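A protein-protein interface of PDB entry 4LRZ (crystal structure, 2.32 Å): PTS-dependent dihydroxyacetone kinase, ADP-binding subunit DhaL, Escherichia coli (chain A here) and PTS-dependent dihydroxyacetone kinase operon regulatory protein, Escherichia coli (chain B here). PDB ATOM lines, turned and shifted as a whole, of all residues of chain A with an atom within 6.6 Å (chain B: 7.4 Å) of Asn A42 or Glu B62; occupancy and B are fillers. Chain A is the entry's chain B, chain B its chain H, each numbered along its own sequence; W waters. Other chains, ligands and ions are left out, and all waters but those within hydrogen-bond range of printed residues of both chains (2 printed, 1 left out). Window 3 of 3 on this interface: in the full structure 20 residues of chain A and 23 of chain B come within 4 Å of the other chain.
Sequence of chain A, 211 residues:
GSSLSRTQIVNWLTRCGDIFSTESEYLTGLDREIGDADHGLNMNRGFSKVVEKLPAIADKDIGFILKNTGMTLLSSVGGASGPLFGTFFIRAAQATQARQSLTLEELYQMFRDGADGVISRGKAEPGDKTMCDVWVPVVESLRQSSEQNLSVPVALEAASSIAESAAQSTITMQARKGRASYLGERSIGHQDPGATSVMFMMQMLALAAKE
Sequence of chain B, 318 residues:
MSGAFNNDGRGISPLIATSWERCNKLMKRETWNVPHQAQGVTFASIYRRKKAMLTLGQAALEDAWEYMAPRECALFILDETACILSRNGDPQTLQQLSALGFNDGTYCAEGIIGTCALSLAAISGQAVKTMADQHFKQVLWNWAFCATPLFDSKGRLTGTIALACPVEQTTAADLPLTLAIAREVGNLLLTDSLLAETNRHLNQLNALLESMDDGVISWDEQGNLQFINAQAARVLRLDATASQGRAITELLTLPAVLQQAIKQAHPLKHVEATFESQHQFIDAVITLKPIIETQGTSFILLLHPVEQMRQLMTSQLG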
ATOM      1  N   SER A  24      -4.210   8.647 -22.130  1.00  0.00           N
ATOM      2  CA  SER A  24      -3.173   7.825 -21.533  1.00  0.00           C
ATOM      3  C   SER A  24      -3.629   7.076 -20.237  1.00  0.00           C
ATOM      4  O   SER A  24      -3.346   5.878 -20.041  1.00  0.00           O
ATOM      5  CB  SER A  24      -1.974   8.707 -21.246  1.00  0.00           C
ATOM      6  OG  SER A  24      -0.899   7.915 -20.845  1.00  0.00           O
ATOM      7  N   THR A  28      -4.045   2.990 -19.741  1.00  0.00           N
ATOM      8  CA  THR A  28      -3.345   2.377 -18.628  1.00  0.00           C
ATOM      9  C   THR A  28      -4.314   1.759 -17.600  1.00  0.00           C
ATOM     10  O   THR A  28      -4.043   0.689 -17.067  1.00  0.00           O
ATOM     11  CB  THR A  28      -2.490   3.425 -17.986  1.00  0.00           C
ATOM     12  OG1 THR A  28      -1.569   3.890 -18.975  1.00  0.00           O
ATOM     13  CG2 THR A  28      -1.714   2.904 -16.747  1.00  0.00           C
ATOM     14  N   ASP A  36      -0.369  -5.358 -17.073  1.00  0.00           N
ATOM     15  CA  ASP A  36       0.644  -4.835 -16.191  1.00  0.00           C
ATOM     16  C   ASP A  36       0.575  -3.325 -16.110  1.00  0.00           C
ATOM     17  O   ASP A  36       1.567  -2.683 -15.762  1.00  0.00           O
ATOM     18  CB  ASP A  36       2.022  -5.322 -16.638  1.00  0.00           C
ATOM     19  CG  ASP A  36       2.412  -4.810 -18.043  1.00  0.00           C
ATOM     20  OD1 ASP A  36       3.501  -5.188 -18.519  1.00  0.00           O
ATOM     21  OD2 ASP A  36       1.635  -4.039 -18.666  1.00  0.00           O
ATOM     22  N   ASP A  38       0.469  -0.540 -18.108  1.00  0.00           N
ATOM     23  CA  ASP A  38       1.459   0.325 -18.797  1.00  0.00           C
ATOM     24  C   ASP A  38       1.023   0.789 -20.182  1.00  0.00           C
ATOM     25  O   ASP A  38       1.656   1.653 -20.773  1.00  0.00           O
ATOM     26  CB  ASP A  38       2.818  -0.390 -18.908  1.00  0.00           C
ATOM     27  CG  ASP A  38       2.754  -1.658 -19.748  1.00  0.00           C
ATOM     28  OD1 ASP A  38       1.762  -1.851 -20.489  1.00  0.00           O
ATOM     29  OD2 ASP A  38       3.719  -2.464 -19.701  1.00  0.00           O
ATOM     30  N   HIS A  39      -0.063   0.239 -20.699  1.00  0.00           N
ATOM     31  CA  HIS A  39      -0.334   0.387 -22.124  1.00  0.00           C
ATOM     32  C   HIS A  39      -0.592   1.810 -22.592  1.00  0.00           C
ATOM     33  O   HIS A  39      -0.114   2.222 -23.650  1.00  0.00           O
ATOM     34  CB  HIS A  39      -1.445  -0.535 -22.580  1.00  0.00           C
ATOM     35  CG  HIS A  39      -1.806  -0.373 -24.029  1.00  0.00           C
ATOM     36  ND1 HIS A  39      -1.006  -0.833 -25.048  1.00  0.00           N
ATOM     37  CD2 HIS A  39      -2.890   0.180 -24.626  1.00  0.00           C
ATOM     38  CE1 HIS A  39      -1.579  -0.570 -26.209  1.00  0.00           C
ATOM     39  NE2 HIS A  39      -2.719   0.047 -25.984  1.00  0.00           N
ATOM     40  N   GLY A  40      -1.322   2.586 -21.808  1.00  0.00           N
ATOM     41  CA  GLY A  40      -1.422   4.009 -22.104  1.00  0.00           C
ATOM     42  C   GLY A  40      -0.097   4.756 -21.997  1.00  0.00           C
ATOM     43  O   GLY A  40       0.261   5.538 -22.878  1.00  0.00           O
ATOM     44  N   LEU A  41       0.634   4.528 -20.921  1.00  0.00           N
ATOM     45  CA  LEU A  41       1.948   5.166 -20.764  1.00  0.00           C
ATOM     46  C   LEU A  41       2.831   4.892 -22.005  1.00  0.00           C
ATOM     47  O   LEU A  41       3.501   5.804 -22.525  1.00  0.00           O
ATOM     48  CB  LEU A  41       2.661   4.681 -19.497  1.00  0.00           C
ATOM     49  CG  LEU A  41       2.062   5.008 -18.118  1.00  0.00           C
ATOM     50  CD1 LEU A  41       2.613   4.075 -16.965  1.00  0.00           C
ATOM     51  CD2 LEU A  41       2.339   6.506 -17.828  1.00  0.00           C
ATOM     52  N   ASN A  42       2.837   3.643 -22.454  1.00  0.00           N
ATOM     53  CA  ASN A  42       3.736   3.235 -23.525  1.00  0.00           C
ATOM     54  C   ASN A  42       3.342   3.747 -24.908  1.00  0.00           C
ATOM     55  O   ASN A  42       4.197   4.107 -25.682  1.00  0.00           O
ATOM     56  CB  ASN A  42       3.935   1.721 -23.526  1.00  0.00           C
ATOM     57  CG  ASN A  42       4.725   1.261 -22.316  1.00  0.00           C
ATOM     58  OD1 ASN A  42       4.903   0.071 -22.082  1.00  0.00           O
ATOM     59  ND2 ASN A  42       5.265   2.225 -21.575  1.00  0.00           N
ATOM     60  N   MET A  43       2.052   3.783 -25.200  1.00  0.00           N
ATOM     61  CA  MET A  43       1.568   4.295 -26.477  1.00  0.00           C
ATOM     62  C   MET A  43       1.866   5.784 -26.561  1.00  0.00           C
ATOM     63  O   MET A  43       2.116   6.331 -27.650  1.00  0.00           O
ATOM     64  CB  MET A  43       0.076   4.009 -26.641  1.00  0.00           C
ATOM     65  CG  MET A  43      -0.250   2.528 -26.844  1.00  0.00           C
ATOM     66  SD  MET A  43       0.435   1.902 -28.415  1.00  0.00           S
ATOM     67  CE  MET A  43      -0.738   2.691 -29.554  1.00  0.00           C
ATOM     68  N   ASN A  44       1.925   6.426 -25.408  1.00  0.00           N
ATOM     69  CA  ASN A  44       2.163   7.840 -25.364  1.00  0.00           C
ATOM     70  C   ASN A  44       3.647   8.123 -25.533  1.00  0.00           C
ATOM     71  O   ASN A  44       4.036   9.073 -26.165  1.00  0.00           O
ATOM     72  CB  ASN A  44       1.646   8.427 -24.031  1.00  0.00           C
ATOM     73  CG  ASN A  44       1.800   9.963 -23.947  1.00  0.00           C
ATOM     74  OD1 ASN A  44       1.630  10.694 -24.933  1.00  0.00           O
ATOM     75  ND2 ASN A  44       2.114  10.439 -22.772  1.00  0.00           N
ATOM     76  N   ARG A  45       4.488   7.303 -24.933  1.00  0.00           N
ATOM     77  CA  ARG A  45       5.898   7.376 -25.164  1.00  0.00           C
ATOM     78  C   ARG A  45       6.180   7.215 -26.683  1.00  0.00           C
ATOM     79  O   ARG A  45       6.941   7.963 -27.271  1.00  0.00           O
ATOM     80  CB  ARG A  45       6.515   6.255 -24.357  1.00  0.00           C
ATOM     81  CG  ARG A  45       8.044   6.075 -24.533  1.00  0.00           C
ATOM     82  CD  ARG A  45       8.593   5.129 -23.475  1.00  0.00           C
ATOM     83  NE  ARG A  45       8.231   3.718 -23.659  1.00  0.00           N
ATOM     84  CZ  ARG A  45       8.398   2.785 -22.708  1.00  0.00           C
ATOM     85  NH1 ARG A  45       8.891   3.115 -21.505  1.00  0.00           N
ATOM     86  NH2 ARG A  45       8.064   1.527 -22.927  1.00  0.00           N
ATOM     87  N   GLY A  46       5.552   6.226 -27.313  1.00  0.00           N
ATOM     88  CA  GLY A  46       5.778   5.925 -28.711  1.00  0.00           C
ATOM     89  C   GLY A  46       5.269   7.030 -29.599  1.00  0.00           C
ATOM     90  O   GLY A  46       6.011   7.639 -30.321  1.00  0.00           O
ATOM     91  N   PHE A  47       3.996   7.328 -29.486  1.00  0.00           N
ATOM     92  CA  PHE A  47       3.399   8.346 -30.302  1.00  0.00           C
ATOM     93  C   PHE A  47       3.904   9.753 -30.071  1.00  0.00           C
ATOM     94  O   PHE A  47       3.917  10.554 -31.025  1.00  0.00           O
ATOM     95  CB  PHE A  47       1.880   8.266 -30.253  1.00  0.00           C
ATOM     96  CG  PHE A  47       1.315   7.437 -31.340  1.00  0.00           C
ATOM     97  CD1 PHE A  47       0.921   6.132 -31.106  1.00  0.00           C
ATOM     98  CD2 PHE A  47       1.234   7.946 -32.658  1.00  0.00           C
ATOM     99  CE1 PHE A  47       0.405   5.360 -32.173  1.00  0.00           C
ATOM    100  CE2 PHE A  47       0.742   7.190 -33.686  1.00  0.00           C
ATOM    101  CZ  PHE A  47       0.338   5.907 -33.454  1.00  0.00           C
ATOM    102  N   LEU A  73       7.549   3.474 -33.581  1.00  0.00           N
ATOM    103  CA  LEU A  73       6.671   2.716 -32.682  1.00  0.00           C
ATOM    104  C   LEU A  73       7.358   1.431 -32.313  1.00  0.00           C
ATOM    105  O   LEU A  73       7.333   1.009 -31.156  1.00  0.00           O
ATOM    106  CB  LEU A  73       5.312   2.417 -33.318  1.00  0.00           C
ATOM    107  CG  LEU A  73       4.540   3.710 -33.516  1.00  0.00           C
ATOM    108  CD1 LEU A  73       3.215   3.367 -34.060  1.00  0.00           C
ATOM    109  CD2 LEU A  73       4.438   4.499 -32.226  1.00  0.00           C
ATOM    110  N   SER A  76      10.197   1.940 -29.410  1.00  0.00           N
ATOM    111  CA  SER A  76      10.005   2.873 -28.331  1.00  0.00           C
ATOM    112  C   SER A  76       8.722   2.640 -27.475  1.00  0.00           C
ATOM    113  O   SER A  76       8.617   3.207 -26.377  1.00  0.00           O
ATOM    114  CB  SER A  76      10.074   4.294 -28.882  1.00  0.00           C
ATOM    115  OG  SER A  76       8.763   4.677 -29.160  1.00  0.00           O
ATOM    116  N   VAL A  77       7.791   1.802 -27.973  1.00  0.00           N
ATOM    117  CA  VAL A  77       6.610   1.381 -27.235  1.00  0.00           C
ATOM    118  C   VAL A  77       6.903   0.221 -26.250  1.00  0.00           C
ATOM    119  O   VAL A  77       6.567   0.313 -25.039  1.00  0.00           O
ATOM    120  CB  VAL A  77       5.423   1.052 -28.183  1.00  0.00           C
ATOM    121  CG1 VAL A  77       4.215   0.612 -27.379  1.00  0.00           C
ATOM    122  CG2 VAL A  77       5.037   2.287 -29.022  1.00  0.00           C
ATOM    123  N   GLY A  78       7.565  -0.837 -26.730  1.00  0.00           N
ATOM    124  CA  GLY A  78       7.893  -2.028 -25.915  1.00  0.00           C
ATOM    125  C   GLY A  78       6.717  -2.992 -25.754  1.00  0.00           C
ATOM    126  O   GLY A  78       5.585  -2.679 -26.135  1.00  0.00           O
ATOM    127  N   GLY A  79       6.989  -4.138 -25.144  1.00  0.00           N
ATOM    128  CA  GLY A  79       6.018  -5.153 -24.794  1.00  0.00           C
ATOM    129  C   GLY A  79       5.403  -5.805 -26.018  1.00  0.00           C
ATOM    130  O   GLY A  79       5.960  -5.787 -27.098  1.00  0.00           O
ATOM    131  N   SER A  81       2.661  -4.860 -27.664  1.00  0.00           N
ATOM    132  CA  SER A  81       1.962  -4.044 -28.665  1.00  0.00           C
ATOM    133  C   SER A  81       2.869  -3.216 -29.592  1.00  0.00           C
ATOM    134  O   SER A  81       2.483  -2.886 -30.722  1.00  0.00           O
ATOM    135  CB  SER A  81       0.907  -3.175 -27.985  1.00  0.00           C
ATOM    136  OG  SER A  81       1.559  -2.148 -27.300  1.00  0.00           O
ATOM    137  N   ARG A 179      -0.657 -10.848 -22.107  1.00  0.00           N
ATOM    138  CA  ARG A 179      -0.616 -10.872 -20.650  1.00  0.00           C
ATOM    139  C   ARG A 179      -1.980 -11.142 -19.995  1.00  0.00           C
ATOM    140  O   ARG A 179      -2.062 -11.805 -18.960  1.00  0.00           O
ATOM    141  CB  ARG A 179      -0.080  -9.548 -20.146  1.00  0.00           C
ATOM    142  CG  ARG A 179       1.412  -9.386 -20.281  1.00  0.00           C
ATOM    143  CD  ARG A 179       1.780  -8.235 -19.393  1.00  0.00           C
ATOM    144  NE  ARG A 179       3.186  -8.164 -19.131  1.00  0.00           N
ATOM    145  CZ  ARG A 179       3.828  -8.806 -18.168  1.00  0.00           C
ATOM    146  NH1 ARG A 179       3.196  -9.623 -17.341  1.00  0.00           N
ATOM    147  NH2 ARG A 179       5.133  -8.627 -18.057  1.00  0.00           N
ATOM    148  N   THR B  55      14.337   6.762 -23.988  1.00  0.00           N
ATOM    149  CA  THR B  55      13.090   6.115 -24.307  1.00  0.00           C
ATOM    150  C   THR B  55      13.357   4.731 -24.907  1.00  0.00           C
ATOM    151  O   THR B  55      12.604   3.791 -24.660  1.00  0.00           O
ATOM    152  CB  THR B  55      12.219   6.944 -25.231  1.00  0.00           C
ATOM    153  OG1 THR B  55      12.767   6.867 -26.534  1.00  0.00           O
ATOM    154  CG2 THR B  55      12.179   8.425 -24.792  1.00  0.00           C
ATOM    155  N   LEU B  56      14.443   4.615 -25.656  1.00  0.00           N
ATOM    156  CA  LEU B  56      14.851   3.353 -26.245  1.00  0.00           C
ATOM    157  C   LEU B  56      15.282   2.422 -25.133  1.00  0.00           C
ATOM    158  O   LEU B  56      14.835   1.273 -25.042  1.00  0.00           O
ATOM    159  CB  LEU B  56      15.971   3.580 -27.251  1.00  0.00           C
ATOM    160  CG  LEU B  56      15.606   4.411 -28.495  1.00  0.00           C
ATOM    161  CD1 LEU B  56      16.828   4.682 -29.370  1.00  0.00           C
ATOM    162  CD2 LEU B  56      14.565   3.697 -29.376  1.00  0.00           C
ATOM    163  N   GLY B  57      16.091   2.929 -24.220  1.00  0.00           N
ATOM    164  CA  GLY B  57      16.538   2.109 -23.114  1.00  0.00           C
ATOM    165  C   GLY B  57      15.459   1.617 -22.167  1.00  0.00           C
ATOM    166  O   GLY B  57      15.543   0.484 -21.690  1.00  0.00           O
ATOM    167  N   GLN B  58      14.451   2.453 -21.893  1.00  0.00           N
ATOM    168  CA  GLN B  58      13.346   2.089 -21.005  1.00  0.00           C
ATOM    169  C   GLN B  58      12.485   0.940 -21.605  1.00  0.00           C
ATOM    170  O   GLN B  58      12.052   0.044 -20.873  1.00  0.00           O
ATOM    171  CB  GLN B  58      12.472   3.322 -20.712  1.00  0.00           C
ATOM    172  CG  GLN B  58      13.122   4.267 -19.720  1.00  0.00           C
ATOM    173  CD  GLN B  58      12.370   5.571 -19.471  1.00  0.00           C
ATOM    174  OE1 GLN B  58      12.371   6.084 -18.335  1.00  0.00           O
ATOM    175  NE2 GLN B  58      11.735   6.127 -20.512  1.00  0.00           N
ATOM    176  N   ALA B  59      12.259   0.958 -22.921  1.00  0.00           N
ATOM    177  CA  ALA B  59      11.447  -0.075 -23.566  1.00  0.00           C
ATOM    178  C   ALA B  59      12.198  -1.398 -23.520  1.00  0.00           C
ATOM    179  O   ALA B  59      11.633  -2.431 -23.160  1.00  0.00           O
ATOM    180  CB  ALA B  59      11.131   0.300 -25.010  1.00  0.00           C
ATOM    181  N   ALA B  60      13.486  -1.338 -23.862  1.00  0.00           N
ATOM    182  CA  ALA B  60      14.374  -2.496 -23.831  1.00  0.00           C
ATOM    183  C   ALA B  60      14.485  -3.107 -22.442  1.00  0.00           C
ATOM    184  O   ALA B  60      14.548  -4.328 -22.296  1.00  0.00           O
ATOM    185  CB  ALA B  60      15.746  -2.092 -24.303  1.00  0.00           C
ATOM    186  N   LEU B  61      14.513  -2.260 -21.427  1.00  0.00           N
ATOM    187  CA  LEU B  61      14.706  -2.715 -20.062  1.00  0.00           C
ATOM    188  C   LEU B  61      13.431  -3.271 -19.500  1.00  0.00           C
ATOM    189  O   LEU B  61      13.474  -4.271 -18.797  1.00  0.00           O
ATOM    190  CB  LEU B  61      15.232  -1.576 -19.159  1.00  0.00           C
ATOM    191  CG  LEU B  61      16.675  -1.763 -18.710  1.00  0.00           C
ATOM    192  CD1 LEU B  61      17.591  -2.354 -19.727  1.00  0.00           C
ATOM    193  CD2 LEU B  61      17.340  -0.480 -18.085  1.00  0.00           C
ATOM    194  N   GLU B  62      12.308  -2.603 -19.751  1.00  0.00           N
ATOM    195  CA  GLU B  62      11.019  -3.204 -19.457  1.00  0.00           C
ATOM    196  C   GLU B  62      10.885  -4.609 -20.082  1.00  0.00           C
ATOM    197  O   GLU B  62      10.518  -5.549 -19.382  1.00  0.00           O
ATOM    198  CB  GLU B  62       9.856  -2.324 -19.920  1.00  0.00           C
ATOM    199  CG  GLU B  62       9.796  -0.994 -19.143  1.00  0.00           C
ATOM    200  CD  GLU B  62       9.026   0.061 -19.916  1.00  0.00           C
ATOM    201  OE1 GLU B  62       8.963   1.234 -19.447  1.00  0.00           O
ATOM    202  OE2 GLU B  62       8.483  -0.302 -21.005  1.00  0.00           O
ATOM    203  N   ASP B  63      11.198  -4.746 -21.367  1.00  0.00           N
ATOM    204  CA  ASP B  63      11.192  -6.057 -22.014  1.00  0.00           C
ATOM    205  C   ASP B  63      12.103  -7.060 -21.331  1.00  0.00           C
ATOM    206  O   ASP B  63      11.649  -8.151 -21.018  1.00  0.00           O
ATOM    207  CB  ASP B  63      11.534  -5.957 -23.504  1.00  0.00           C
ATOM    208  CG  ASP B  63      10.431  -5.253 -24.309  1.00  0.00           C
ATOM    209  OD1 ASP B  63      10.531  -5.178 -25.559  1.00  0.00           O
ATOM    210  OD2 ASP B  63       9.447  -4.754 -23.714  1.00  0.00           O
ATOM    211  N   ALA B  64      13.366  -6.705 -21.077  1.00  0.00           N
ATOM    212  CA  ALA B  64      14.276  -7.625 -20.395  1.00  0.00           C
ATOM    213  C   ALA B  64      13.660  -8.070 -19.059  1.00  0.00           C
ATOM    214  O   ALA B  64      13.739  -9.240 -18.705  1.00  0.00           O
ATOM    215  CB  ALA B  64      15.617  -6.989 -20.156  1.00  0.00           C
ATOM    216  N   TRP B  65      13.044  -7.150 -18.323  1.00  0.00           N
ATOM    217  CA  TRP B  65      12.474  -7.514 -17.019  1.00  0.00           C
ATOM    218  C   TRP B  65      11.361  -8.570 -17.130  1.00  0.00           C
ATOM    219  O   TRP B  65      11.408  -9.597 -16.465  1.00  0.00           O
ATOM    220  CB  TRP B  65      12.014  -6.262 -16.249  1.00  0.00           C
ATOM    221  CG  TRP B  65      11.305  -6.563 -14.973  1.00  0.00           C
ATOM    222  CD1 TRP B  65      10.030  -6.188 -14.638  1.00  0.00           C
ATOM    223  CD2 TRP B  65      11.807  -7.316 -13.871  1.00  0.00           C
ATOM    224  NE1 TRP B  65       9.714  -6.653 -13.395  1.00  0.00           N
ATOM    225  CE2 TRP B  65      10.781  -7.355 -12.894  1.00  0.00           C
ATOM    226  CE3 TRP B  65      13.017  -7.971 -13.611  1.00  0.00           C
ATOM    227  CZ2 TRP B  65      10.921  -8.038 -11.668  1.00  0.00           C
ATOM    228  CZ3 TRP B  65      13.149  -8.663 -12.398  1.00  0.00           C
ATOM    229  CH2 TRP B  65      12.100  -8.688 -11.443  1.00  0.00           C
ATOM    230  N   GLU B  66      10.372  -8.297 -17.961  1.00  0.00           N
ATOM    231  CA  GLU B  66       9.277  -9.199 -18.233  1.00  0.00           C
ATOM    232  C   GLU B  66       9.689 -10.646 -18.553  1.00  0.00           C
ATOM    233  O   GLU B  66       9.096 -11.564 -18.040  1.00  0.00           O
ATOM    234  CB  GLU B  66       8.420  -8.642 -19.368  1.00  0.00           C
ATOM    235  CG  GLU B  66       7.613  -9.722 -20.090  1.00  0.00           C
ATOM    236  CD  GLU B  66       6.716  -9.211 -21.223  1.00  0.00           C
ATOM    237  OE1 GLU B  66       5.641  -9.840 -21.482  1.00  0.00           O
ATOM    238  OE2 GLU B  66       7.093  -8.205 -21.867  1.00  0.00           O
ATOM    239  N   TYR B  67      10.688 -10.860 -19.405  1.00  0.00           N
ATOM    240  CA  TYR B  67      11.081 -12.232 -19.750  1.00  0.00           C
ATOM    241  C   TYR B  67      11.986 -12.876 -18.701  1.00  0.00           C
ATOM    242  O   TYR B  67      12.352 -14.051 -18.826  1.00  0.00           O
ATOM    243  CB  TYR B  67      11.665 -12.288 -21.176  1.00  0.00           C
ATOM    244  CG  TYR B  67      10.558 -12.134 -22.168  1.00  0.00           C
ATOM    245  CD1 TYR B  67       9.833 -13.235 -22.597  1.00  0.00           C
ATOM    246  CD2 TYR B  67      10.159 -10.883 -22.594  1.00  0.00           C
ATOM    247  CE1 TYR B  67       8.793 -13.108 -23.456  1.00  0.00           C
ATOM    248  CE2 TYR B  67       9.102 -10.742 -23.474  1.00  0.00           C
ATOM    249  CZ  TYR B  67       8.431 -11.862 -23.890  1.00  0.00           C
ATOM    250  OH  TYR B  67       7.384 -11.726 -24.743  1.00  0.00           O
ATOM    251  N   MET B  68      12.280 -12.109 -17.647  1.00  0.00           N
ATOM    252  CA  MET B  68      13.173 -12.501 -16.552  1.00  0.00           C
ATOM    253  C   MET B  68      12.460 -12.664 -15.196  1.00  0.00           C
ATOM    254  O   MET B  68      12.913 -13.416 -14.339  1.00  0.00           O
ATOM    255  CB  MET B  68      14.305 -11.459 -16.450  1.00  0.00           C
ATOM    256  CG  MET B  68      15.198 -11.499 -15.248  1.00  0.00           C
ATOM    257  SD  MET B  68      16.720 -10.569 -15.560  1.00  0.00           S
ATOM    258  CE  MET B  68      17.592 -11.969 -16.150  1.00  0.00           C
ATOM    259  N   LEU B  75      17.417  -3.190 -12.737  1.00  0.00           N
ATOM    260  CA  LEU B  75      18.045  -2.707 -13.961  1.00  0.00           C
ATOM    261  C   LEU B  75      18.120  -1.147 -13.942  1.00  0.00           C
ATOM    262  O   LEU B  75      17.122  -0.463 -13.606  1.00  0.00           O
ATOM    263  CB  LEU B  75      17.232  -3.191 -15.143  1.00  0.00           C
ATOM    264  CG  LEU B  75      17.081  -4.720 -15.252  1.00  0.00           C
ATOM    265  CD1 LEU B  75      16.030  -5.022 -16.295  1.00  0.00           C
ATOM    266  CD2 LEU B  75      18.373  -5.406 -15.611  1.00  0.00           C
ATOM    267  N   SER B  86      16.992   6.096 -14.919  1.00  0.00           N
ATOM    268  CA  SER B  86      15.787   5.266 -14.828  1.00  0.00           C
ATOM    269  C   SER B  86      16.112   3.895 -14.227  1.00  0.00           C
ATOM    270  O   SER B  86      17.190   3.320 -14.496  1.00  0.00           O
ATOM    271  CB  SER B  86      15.146   5.126 -16.215  1.00  0.00           C
ATOM    272  OG  SER B  86      13.887   4.466 -16.142  1.00  0.00           O
ATOM    273  N   ASN B  88      14.245  -0.057 -13.006  1.00  0.00           N
ATOM    274  CA  ASN B  88      13.070  -0.930 -13.086  1.00  0.00           C
ATOM    275  C   ASN B  88      13.490  -2.322 -12.684  1.00  0.00           C
ATOM    276  O   ASN B  88      14.670  -2.554 -12.458  1.00  0.00           O
ATOM    277  CB  ASN B  88      12.373  -0.887 -14.467  1.00  0.00           C
ATOM    278  CG  ASN B  88      13.095  -1.690 -15.506  1.00  0.00           C
ATOM    279  OD1 ASN B  88      12.524  -2.622 -16.080  1.00  0.00           O
ATOM    280  ND2 ASN B  88      14.357  -1.393 -15.723  1.00  0.00           N
ATOM    281  N   GLY B  89      12.529  -3.226 -12.536  1.00  0.00           N
ATOM    282  CA  GLY B  89      12.830  -4.553 -12.045  1.00  0.00           C
ATOM    283  C   GLY B  89      12.112  -4.817 -10.735  1.00  0.00           C
ATOM    284  O   GLY B  89      10.986  -4.345 -10.513  1.00  0.00           O
HETATM  285  O   HOH W   1       7.567  -2.301 -22.446  1.00  0.00           O
HETATM  286  O   HOH W   2       4.517 -11.525 -18.989  1.00  0.00           O
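Among the printed residues, pairs that only touch across the chains: Arg A45 with Gln B58, Asn A42 with Glu B62, Arg A45 with Ala B59 and Gly A78 with Asp B63.
Water W1 lies within hydrogen-bond range of the side-chain carboxylate of Glu B62, the backbone NH of Gly A79 and the side-chain carboxylate of Asp B63.
Water W2 bridges NH1 of Arg A179 and OE1 of Glu B66.
NH2 of Arg A45 is in salt-bridge range of OE2 of Glu B62 (2.7 Å).
The backbone NH (N) of Gly A79 is in hydrogen-bond range of the side-chain carboxylate (OD2) of Asp B63 (2.9 Å).
The guanidinium group of Arg A179 lies within salt-bridge range of the side-chain carboxylate of Glu B66 (3.7 Å).
The side-chain carboxylate (OD1) of Asp A36 lies close to the guanidinium group (NE) of Arg A179.
The side-chain amide nitrogen (ND2) of Asn A42 sits close to the guanidinium group (NH2) of Arg A45, at 3.2 Å.
O of Val A77 lies close to OD1 of Asn A42 (3.4 Å).
O of Ser A76 is in hydrogen-bond range of NE of Arg A45, at 2.8 Å.
NH2 of Arg A45 sits at hydrogen-bond distance from O of Val A77 (2.9 Å).
The side-chain hydroxyl of Ser B86 lies within hydrogen-bond range of the side-chain amide oxygen of Gln B58, at 3.1 Å.
Asn A42 touches one residue of chain B.
Glu B62 touches just these residues of chain A: Asn A42 (3.8 Å) and Arg A45 (2.7 Å).
Printed residues of chain A within 4 Å of Gln B58: Arg A45.
Of the printed residues of chain B, Gly A78 touches Asp B63 (3.8 Å).
Printed residues of chain B within 4 Å of Arg A45: Gln B58, Ala B59 and Glu B62.
The nearest printed residue of chain B that does not touch Arg A45 is Thr B55 (4.3 Å).
Among the printed residues, Asp or Glu carboxylates within 4 Å of a Lys or Arg side-chain nitrogen of the other chain: Arg A45 with Glu B62 (2.7 Å) and Arg A179 with Glu B66 (3.7 Å).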
